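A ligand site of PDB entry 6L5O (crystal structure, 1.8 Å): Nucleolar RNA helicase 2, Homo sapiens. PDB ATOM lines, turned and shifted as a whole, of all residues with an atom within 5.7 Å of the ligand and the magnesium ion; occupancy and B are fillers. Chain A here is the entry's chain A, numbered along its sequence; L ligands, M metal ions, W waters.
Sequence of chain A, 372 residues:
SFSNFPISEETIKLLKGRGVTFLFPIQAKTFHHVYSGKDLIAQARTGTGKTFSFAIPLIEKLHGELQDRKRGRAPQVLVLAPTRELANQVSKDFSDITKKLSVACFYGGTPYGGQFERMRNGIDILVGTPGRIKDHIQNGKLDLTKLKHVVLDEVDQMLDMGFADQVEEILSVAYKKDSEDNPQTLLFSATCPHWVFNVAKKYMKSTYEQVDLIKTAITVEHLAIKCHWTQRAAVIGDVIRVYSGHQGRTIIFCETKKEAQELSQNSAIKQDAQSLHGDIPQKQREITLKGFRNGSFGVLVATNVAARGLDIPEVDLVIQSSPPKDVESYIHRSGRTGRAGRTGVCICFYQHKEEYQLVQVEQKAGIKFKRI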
ATOM      1  N   ARG A  18      22.305   3.309  11.419  1.00  0.00           N
ATOM      2  CA  ARG A  18      21.922   3.743  10.092  1.00  0.00           C
ATOM      3  C   ARG A  18      20.801   4.774  10.119  1.00  0.00           C
ATOM      4  O   ARG A  18      20.191   5.036   9.077  1.00  0.00           O
ATOM      5  CB  ARG A  18      21.500   2.528   9.253  1.00  0.00           C
ATOM      6  CG  ARG A  18      22.670   1.585   8.937  1.00  0.00           C
ATOM      7  CD  ARG A  18      23.716   2.252   8.021  1.00  0.00           C
ATOM      8  NE  ARG A  18      23.076   2.835   6.843  1.00  0.00           N
ATOM      9  CZ  ARG A  18      22.813   2.170   5.717  1.00  0.00           C
ATOM     10  NH1 ARG A  18      23.161   0.893   5.600  1.00  0.00           N
ATOM     11  NH2 ARG A  18      22.200   2.770   4.701  1.00  0.00           N
ATOM     12  N   GLY A  19      20.522   5.363  11.283  1.00  0.00           N
ATOM     13  CA  GLY A  19      19.453   6.344  11.372  1.00  0.00           C
ATOM     14  C   GLY A  19      18.052   5.802  11.276  1.00  0.00           C
ATOM     15  O   GLY A  19      17.114   6.573  11.077  1.00  0.00           O
ATOM     16  N   VAL A  20      17.864   4.501  11.418  1.00  0.00           N
ATOM     17  CA  VAL A  20      16.534   3.882  11.300  1.00  0.00           C
ATOM     18  C   VAL A  20      15.982   3.680  12.707  1.00  0.00           C
ATOM     19  O   VAL A  20      16.528   2.882  13.482  1.00  0.00           O
ATOM     20  CB  VAL A  20      16.623   2.550  10.536  1.00  0.00           C
ATOM     21  CG1 VAL A  20      15.241   1.883  10.497  1.00  0.00           C
ATOM     22  CG2 VAL A  20      17.177   2.764   9.136  1.00  0.00           C
ATOM     23  N   THR A  21      14.896   4.386  13.047  1.00  0.00           N
ATOM     24  CA  THR A  21      14.269   4.235  14.364  1.00  0.00           C
ATOM     25  C   THR A  21      12.817   3.790  14.311  1.00  0.00           C
ATOM     26  O   THR A  21      12.234   3.525  15.364  1.00  0.00           O
ATOM     27  CB  THR A  21      14.330   5.562  15.167  1.00  0.00           C
ATOM     28  OG1 THR A  21      13.619   6.587  14.472  1.00  0.00           O
ATOM     29  CG2 THR A  21      15.758   5.987  15.373  1.00  0.00           C
ATOM     30  N   PHE A  22      12.222   3.692  13.122  1.00  0.00           N
ATOM     31  CA  PHE A  22      10.896   3.123  12.945  1.00  0.00           C
ATOM     32  C   PHE A  22      10.785   2.692  11.485  1.00  0.00           C
ATOM     33  O   PHE A  22      11.576   3.114  10.645  1.00  0.00           O
ATOM     34  CB  PHE A  22       9.798   4.119  13.325  1.00  0.00           C
ATOM     35  CG  PHE A  22       9.668   5.284  12.375  1.00  0.00           C
ATOM     36  CD1 PHE A  22      10.409   6.427  12.567  1.00  0.00           C
ATOM     37  CD2 PHE A  22       8.795   5.221  11.292  1.00  0.00           C
ATOM     38  CE1 PHE A  22      10.295   7.497  11.706  1.00  0.00           C
ATOM     39  CE2 PHE A  22       8.678   6.300  10.417  1.00  0.00           C
ATOM     40  CZ  PHE A  22       9.431   7.431  10.627  1.00  0.00           C
ATOM     41  N   LEU A  23       9.775   1.884  11.193  1.00  0.00           N
ATOM     42  CA  LEU A  23       9.623   1.363   9.840  1.00  0.00           C
ATOM     43  C   LEU A  23       8.746   2.295   8.996  1.00  0.00           C
ATOM     44  O   LEU A  23       7.651   2.674   9.421  1.00  0.00           O
ATOM     45  CB  LEU A  23       9.024  -0.050   9.858  1.00  0.00           C
ATOM     46  CG  LEU A  23       9.843  -1.201  10.480  1.00  0.00           C
ATOM     47  CD1 LEU A  23       9.150  -2.543  10.226  1.00  0.00           C
ATOM     48  CD2 LEU A  23      11.299  -1.257   9.968  1.00  0.00           C
ATOM     49  N   PHE A  24       9.253   2.669   7.813  1.00  0.00           N
ATOM     50  CA  PHE A  24       8.463   3.399   6.820  1.00  0.00           C
ATOM     51  C   PHE A  24       7.277   2.555   6.368  1.00  0.00           C
ATOM     52  O   PHE A  24       7.265   1.339   6.556  1.00  0.00           O
ATOM     53  CB  PHE A  24       9.343   3.743   5.616  1.00  0.00           C
ATOM     54  CG  PHE A  24      10.376   4.793   5.898  1.00  0.00           C
ATOM     55  CD1 PHE A  24      10.333   5.543   7.063  1.00  0.00           C
ATOM     56  CD2 PHE A  24      11.370   5.057   4.963  1.00  0.00           C
ATOM     57  CE1 PHE A  24      11.274   6.531   7.301  1.00  0.00           C
ATOM     58  CE2 PHE A  24      12.311   6.045   5.201  1.00  0.00           C
ATOM     59  CZ  PHE A  24      12.274   6.783   6.372  1.00  0.00           C
ATOM     60  N   GLN A  27       7.913  -0.649   4.490  1.00  0.00           N
ATOM     61  CA  GLN A  27       8.480  -1.662   5.363  1.00  0.00           C
ATOM     62  C   GLN A  27       7.422  -2.245   6.291  1.00  0.00           C
ATOM     63  O   GLN A  27       7.329  -3.469   6.452  1.00  0.00           O
ATOM     64  CB  GLN A  27       9.628  -1.046   6.174  1.00  0.00           C
ATOM     65  CG  GLN A  27      10.754  -0.653   5.260  1.00  0.00           C
ATOM     66  CD  GLN A  27      11.626   0.488   5.743  1.00  0.00           C
ATOM     67  OE1 GLN A  27      11.455   1.042   6.847  1.00  0.00           O
ATOM     68  NE2 GLN A  27      12.601   0.859   4.898  1.00  0.00           N
ATOM     69  N   ALA A  44       6.639   0.643  -4.566  1.00  0.00           N
ATOM     70  CA  ALA A  44       6.708   1.920  -3.864  1.00  0.00           C
ATOM     71  C   ALA A  44       7.674   2.823  -4.619  1.00  0.00           C
ATOM     72  O   ALA A  44       8.581   2.348  -5.293  1.00  0.00           O
ATOM     73  CB  ALA A  44       7.173   1.748  -2.410  1.00  0.00           C
ATOM     74  N   ARG A  45       7.466   4.130  -4.468  1.00  0.00           N
ATOM     75  CA  ARG A  45       8.277   5.088  -5.202  1.00  0.00           C
ATOM     76  C   ARG A  45       9.752   4.977  -4.816  1.00  0.00           C
ATOM     77  O   ARG A  45      10.114   4.524  -3.736  1.00  0.00           O
ATOM     78  CB  ARG A  45       7.780   6.515  -4.933  1.00  0.00           C
ATOM     79  CG  ARG A  45       6.302   6.703  -5.237  1.00  0.00           C
ATOM     80  CD  ARG A  45       5.783   8.022  -4.677  1.00  0.00           C
ATOM     81  NE  ARG A  45       6.349   9.168  -5.392  1.00  0.00           N
ATOM     82  CZ  ARG A  45       5.870  10.407  -5.282  1.00  0.00           C
ATOM     83  NH1 ARG A  45       4.824  10.634  -4.493  1.00  0.00           N
ATOM     84  NH2 ARG A  45       6.420  11.418  -5.945  1.00  0.00           N
ATOM     85  N   THR A  46      10.609   5.420  -5.735  1.00  0.00           N
ATOM     86  CA  THR A  46      12.033   5.458  -5.454  1.00  0.00           C
ATOM     87  C   THR A  46      12.306   6.311  -4.216  1.00  0.00           C
ATOM     88  O   THR A  46      11.711   7.374  -4.021  1.00  0.00           O
ATOM     89  CB  THR A  46      12.787   5.992  -6.665  1.00  0.00           C
ATOM     90  OG1 THR A  46      12.599   5.094  -7.770  1.00  0.00           O
ATOM     91  CG2 THR A  46      14.282   6.061  -6.367  1.00  0.00           C
ATOM     92  N   GLY A  47      13.173   5.795  -3.352  1.00  0.00           N
ATOM     93  CA  GLY A  47      13.583   6.487  -2.147  1.00  0.00           C
ATOM     94  C   GLY A  47      12.742   6.223  -0.917  1.00  0.00           C
ATOM     95  O   GLY A  47      12.976   6.865   0.112  1.00  0.00           O
ATOM     96  N   THR A  48      11.785   5.307  -0.977  1.00  0.00           N
ATOM     97  CA  THR A  48      10.846   5.115   0.119  1.00  0.00           C
ATOM     98  C   THR A  48      11.207   3.951   1.037  1.00  0.00           C
ATOM     99  O   THR A  48      10.495   3.731   2.023  1.00  0.00           O
ATOM    100  CB  THR A  48       9.409   4.959  -0.395  1.00  0.00           C
ATOM    101  OG1 THR A  48       9.313   3.822  -1.248  1.00  0.00           O
ATOM    102  CG2 THR A  48       8.960   6.211  -1.137  1.00  0.00           C
ATOM    103  N   GLY A  49      12.275   3.209   0.749  1.00  0.00           N
ATOM    104  CA  GLY A  49      12.769   2.235   1.711  1.00  0.00           C
ATOM    105  C   GLY A  49      12.568   0.779   1.330  1.00  0.00           C
ATOM    106  O   GLY A  49      12.398  -0.088   2.206  1.00  0.00           O
ATOM    107  N   LYS A  50      12.587   0.479   0.030  1.00  0.00           N
ATOM    108  CA  LYS A  50      12.336  -0.906  -0.366  1.00  0.00           C
ATOM    109  C   LYS A  50      13.450  -1.834   0.111  1.00  0.00           C
ATOM    110  O   LYS A  50      13.172  -2.992   0.422  1.00  0.00           O
ATOM    111  CB  LYS A  50      12.150  -1.002  -1.880  1.00  0.00           C
ATOM    112  CG  LYS A  50      10.852  -0.294  -2.337  1.00  0.00           C
ATOM    113  CD  LYS A  50      10.489  -0.537  -3.790  1.00  0.00           C
ATOM    114  CE  LYS A  50      11.420   0.224  -4.733  1.00  0.00           C
ATOM    115  NZ  LYS A  50      11.375   1.719  -4.498  1.00  0.00           N
ATOM    116  N   THR A  51      14.701  -1.355   0.203  1.00  0.00           N
ATOM    117  CA  THR A  51      15.788  -2.273   0.540  1.00  0.00           C
ATOM    118  C   THR A  51      15.557  -2.910   1.899  1.00  0.00           C
ATOM    119  O   THR A  51      15.613  -4.144   2.033  1.00  0.00           O
ATOM    120  CB  THR A  51      17.146  -1.564   0.527  1.00  0.00           C
ATOM    121  OG1 THR A  51      17.333  -0.932  -0.743  1.00  0.00           O
ATOM    122  CG2 THR A  51      18.266  -2.595   0.726  1.00  0.00           C
ATOM    123  N   PHE A  52      15.313  -2.102   2.932  1.00  0.00           N
ATOM    124  CA  PHE A  52      15.096  -2.652   4.265  1.00  0.00           C
ATOM    125  C   PHE A  52      13.769  -3.404   4.375  1.00  0.00           C
ATOM    126  O   PHE A  52      13.611  -4.221   5.293  1.00  0.00           O
ATOM    127  CB  PHE A  52      15.152  -1.522   5.294  1.00  0.00           C
ATOM    128  CG  PHE A  52      16.561  -1.098   5.647  1.00  0.00           C
ATOM    129  CD1 PHE A  52      17.569  -2.044   5.737  1.00  0.00           C
ATOM    130  CD2 PHE A  52      16.858   0.231   5.888  1.00  0.00           C
ATOM    131  CE1 PHE A  52      18.874  -1.661   6.069  1.00  0.00           C
ATOM    132  CE2 PHE A  52      18.162   0.620   6.196  1.00  0.00           C
ATOM    133  CZ  PHE A  52      19.168  -0.323   6.295  1.00  0.00           C
ATOM    134  N   LEU A  86      23.856  -0.845  -7.638  1.00  0.00           N
ATOM    135  CA  LEU A  86      22.678  -1.241  -6.866  1.00  0.00           C
ATOM    136  C   LEU A  86      22.946  -2.505  -6.055  1.00  0.00           C
ATOM    137  O   LEU A  86      22.489  -2.621  -4.914  1.00  0.00           O
ATOM    138  CB  LEU A  86      21.493  -1.458  -7.819  1.00  0.00           C
ATOM    139  CG  LEU A  86      20.939  -0.186  -8.462  1.00  0.00           C
ATOM    140  CD1 LEU A  86      19.891  -0.522  -9.505  1.00  0.00           C
ATOM    141  CD2 LEU A  86      20.351   0.723  -7.392  1.00  0.00           C
ATOM    142  N   GLN A  89      24.994  -1.506  -2.977  1.00  0.00           N
ATOM    143  CA  GLN A  89      24.191  -0.813  -1.961  1.00  0.00           C
ATOM    144  C   GLN A  89      23.337  -1.786  -1.178  1.00  0.00           C
ATOM    145  O   GLN A  89      23.209  -1.670   0.050  1.00  0.00           O
ATOM    146  CB  GLN A  89      23.328   0.258  -2.621  1.00  0.00           C
ATOM    147  CG  GLN A  89      22.262   0.858  -1.690  1.00  0.00           C
ATOM    148  CD  GLN A  89      20.843   0.349  -1.996  1.00  0.00           C
ATOM    149  OE1 GLN A  89      20.400   0.354  -3.150  1.00  0.00           O
ATOM    150  NE2 GLN A  89      20.122  -0.084  -0.951  1.00  0.00           N
ATOM    151  N   ASP A  93      23.679  -2.734   2.874  1.00  0.00           N
ATOM    152  CA  ASP A  93      22.575  -2.603   3.811  1.00  0.00           C
ATOM    153  C   ASP A  93      22.367  -3.878   4.621  1.00  0.00           C
ATOM    154  O   ASP A  93      22.109  -3.815   5.825  1.00  0.00           O
ATOM    155  CB  ASP A  93      21.313  -2.167   3.065  1.00  0.00           C
ATOM    156  CG  ASP A  93      21.356  -0.682   2.675  1.00  0.00           C
ATOM    157  OD1 ASP A  93      22.190   0.058   3.261  1.00  0.00           O
ATOM    158  OD2 ASP A  93      20.562  -0.248   1.812  1.00  0.00           O
ATOM    159  N   ASP A 153      15.253  -7.310  -7.172  1.00  0.00           N
ATOM    160  CA  ASP A 153      15.207  -5.913  -6.797  1.00  0.00           C
ATOM    161  C   ASP A 153      15.283  -5.044  -8.043  1.00  0.00           C
ATOM    162  O   ASP A 153      16.072  -5.328  -8.939  1.00  0.00           O
ATOM    163  CB  ASP A 153      16.349  -5.546  -5.840  1.00  0.00           C
ATOM    164  CG  ASP A 153      16.151  -4.186  -5.185  1.00  0.00           C
ATOM    165  OD1 ASP A 153      14.994  -3.740  -5.035  1.00  0.00           O
ATOM    166  OD2 ASP A 153      17.162  -3.549  -4.825  1.00  0.00           O
ATOM    167  N   GLU A 154      14.456  -3.991  -8.083  1.00  0.00           N
ATOM    168  CA  GLU A 154      14.343  -3.146  -9.279  1.00  0.00           C
ATOM    169  C   GLU A 154      14.079  -4.020 -10.497  1.00  0.00           C
ATOM    170  O   GLU A 154      14.751  -3.938 -11.522  1.00  0.00           O
ATOM    171  CB  GLU A 154      15.588  -2.277  -9.492  1.00  0.00           C
ATOM    172  CG  GLU A 154      15.756  -1.112  -8.502  1.00  0.00           C
ATOM    173  CD  GLU A 154      14.553  -0.168  -8.508  1.00  0.00           C
ATOM    174  OE1 GLU A 154      13.810  -0.165  -7.517  1.00  0.00           O
ATOM    175  OE2 GLU A 154      14.335   0.529  -9.528  1.00  0.00           O
HETATM  176  P1  LIG L   1      14.212   2.471  -2.480  1.00  0.00           P
HETATM  177  O1  LIG L   1      12.762   2.411  -2.122  1.00  0.00           O
HETATM  178  O2  LIG L   1      14.573   3.449  -3.586  1.00  0.00           O
HETATM  179  O3  LIG L   1      14.870   1.108  -2.678  1.00  0.00           O
HETATM  180  P2  LIG L   1      16.210   2.621  -0.350  1.00  0.00           P
HETATM  181  O4  LIG L   1      16.031   1.266   0.267  1.00  0.00           O
HETATM  182  O5  LIG L   1      17.394   2.911  -1.237  1.00  0.00           O
HETATM  183  O6  LIG L   1      14.883   3.082  -1.142  1.00  0.00           O
HETATM  184  O7  LIG L   1      16.197   3.707   0.839  1.00  0.00           O
HETATM  185  C1  LIG L   1      16.365   5.097   0.576  1.00  0.00           C
HETATM  186  C2  LIG L   1      17.068   5.740   1.781  1.00  0.00           C
HETATM  187  O8  LIG L   1      16.215   5.767   2.921  1.00  0.00           O
HETATM  188  C3  LIG L   1      18.316   4.980   2.211  1.00  0.00           C
HETATM  189  O9  LIG L   1      19.288   5.943   2.626  1.00  0.00           O
HETATM  190  C4  LIG L   1      17.858   4.213   3.440  1.00  0.00           C
HETATM  191  O10 LIG L   1      18.922   3.854   4.320  1.00  0.00           O
HETATM  192  C5  LIG L   1      16.877   5.196   4.047  1.00  0.00           C
HETATM  193  N1  LIG L   1      15.857   4.492   4.852  1.00  0.00           N
HETATM  194  C6  LIG L   1      15.171   3.392   4.474  1.00  0.00           C
HETATM  195  N2  LIG L   1      14.320   2.992   5.444  1.00  0.00           N
HETATM  196  C7  LIG L   1      14.475   3.874   6.472  1.00  0.00           C
HETATM  197  C8  LIG L   1      13.861   4.049   7.792  1.00  0.00           C
HETATM  198  N3  LIG L   1      12.912   3.200   8.252  1.00  0.00           N
HETATM  199  N4  LIG L   1      14.292   5.098   8.548  1.00  0.00           N
HETATM  200  C9  LIG L   1      15.223   5.947   8.105  1.00  0.00           C
HETATM  201  N5  LIG L   1      15.825   5.860   6.904  1.00  0.00           N
HETATM  202  C10 LIG L   1      15.489   4.854   6.070  1.00  0.00           C
HETATM  203 MG    MG M   1      15.935   0.098  -4.077  1.00  0.00          MG
HETATM  204  O   HOH W   1      15.775   1.773  -5.378  1.00  0.00           O
HETATM  205  O   HOH W   2      19.898   3.786  -1.068  1.00  0.00           O
HETATM  206  O   HOH W   3      18.709   1.067   3.150  1.00  0.00           O
HETATM  207  O   HOH W   4      20.701   4.944   6.202  1.00  0.00           O
HETATM  208  O   HOH W   5      16.242  -1.623  -2.953  1.00  0.00           O
HETATM  209  O   HOH W   6      17.051   4.855  -3.634  1.00  0.00           O
HETATM  210  O   HOH W   7      15.703   0.720   2.804  1.00  0.00           O
HETATM  211  O   HOH W   8      13.578   5.879  10.938  1.00  0.00           O
HETATM  212  O   HOH W   9      14.625  -0.994  -5.070  1.00  0.00           O
HETATM  213  O   HOH W  10      17.565   0.980  -3.112  1.00  0.00           O
HETATM  214  O   HOH W  11      17.598  -0.508  -5.567  1.00  0.00           O
HETATM  215  O   HOH W  12      18.334   7.658   6.571  1.00  0.00           O
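Gly 19 touches the ligand. CG1 of Val 20 touches N3 of the ligand, at 3.5 Å. Phe 24 touches the ligand (CE2 to C7, 3.3 Å). O of Arg 45 touches O1 of the ligand (3.8 Å). Thr 46 touches the ligand (C to O2, 3.7 Å). Phe 52 touches the ligand (CD2 to N2, 3.8 Å). Hydrophobic or aromatic side chains that line the ligand: Val 20, Phe 24 and Phe 52. 14 residues have an atom within 4 Å of the ligand: Arg 18, Gly 19, Val 20, Phe 22, Phe 24, Gln 27, Arg 45, Thr 46, Gly 47, Thr 48, Gly 49, Lys 50, Thr 51 and Phe 52. Along chain A the residues within 4 Å of the ligand span positions 18 to 52.
The magnesium ion is bound by water W9, O3 of the ligand, water W5, water W10, water W1 and water W11. The magnesium ion has six donor atoms within binding distance.
Water W10 lies within hydrogen-bond range of an oxygen (O5) of the ligand (2.7 Å), the side-chain amide oxygen of Gln 89 (2.9 Å) and the side-chain hydroxyl of Thr 51 (3.1 Å). Water W5 bridges OG1 of Thr 51 (2.6 Å) and OD2 of Asp 153 (2.8 Å). Water W9 lies within hydrogen-bond range of the side-chain carboxylate (OE1) of Glu 154 and the side-chain carboxylate (OD1) of Asp 153. Water W8 lies within hydrogen-bond range of N4 of the ligand (2.6 Å), N of Thr 21 (2.9 Å) and N of Phe 22 (3.4 Å). Water W4 lies within hydrogen-bond range of an oxygen (O10) of the ligand (2.8 Å) and the backbone carbonyl oxygen (O) of Arg 18 (2.9 Å). Water W3 bridges the side-chain carboxylate of Asp 93 (2.6 Å) and an oxygen (O10) of the ligand (3.0 Å).
The backbone NH (N) of Gly 47 sits at hydrogen-bond distance from an oxygen (O2) of the ligand, 2.7 Å away. The guanidinium group (NH2) of Arg 18 lies within hydrogen-bond range of an oxygen (O10) of the ligand, at 3.5 Å. N of Lys 50 lies within hydrogen-bond range of O1 of the ligand, at 2.9 Å. The backbone NH (N) of Gly 49 lies within hydrogen-bond range of an oxygen (O1) of the ligand (3.0 Å). O of Phe 22 is in hydrogen-bond range of N3 of the ligand, 2.7 Å away. NZ of Lys 50 is in salt-bridge range of O1 of the ligand (2.8 Å). NE2 of Gln 27 lies within hydrogen-bond range of N2 of the ligand, at 2.8 Å. O4 of the ligand sits at hydrogen-bond distance from N of Thr 51, at 2.9 Å. O4 of the ligand lies within hydrogen-bond range of OG1 of Thr 51, at 2.7 Å. The backbone NH (N) of Thr 48 sits at hydrogen-bond distance from an oxygen (O1) of the ligand.
OG1 of Thr 48 sits at hydrogen-bond distance from O of Arg 45 (2.7 Å). The side-chain amide oxygen (OE1) of Gln 27 is in hydrogen-bond range of the backbone NH (N) of Phe 24, at 2.9 Å. The side-chain amide nitrogen (NE2) of Gln 27 sits at hydrogen-bond distance from the backbone carbonyl oxygen (O) of Gly 49 (2.9 Å). NZ of Lys 50 lies within hydrogen-bond range of O of Arg 45, at 3.2 Å. The side-chain hydroxyl (OG1) of Thr 51 sits at hydrogen-bond distance from the side-chain amide nitrogen (NE2) of Gln 89, at 2.9 Å. The backbone carbonyl oxygen of Ala 44 sits at hydrogen-bond distance from the side-chain amino group of Lys 50 (3.0 Å). NH1 of Arg 18 lies within salt-bridge range of OD1 of Asp 93 (2.7 Å).
Thr 51 touches the magnesium ion. Asp 153 touches the magnesium ion (OD2 to MG, 3.9 Å). Of the 22 residues printed, 2 come within 4 Å of the magnesium ion. The nearest printed residue that does not touch the magnesium ion is Glu 154 (4.1 Å).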
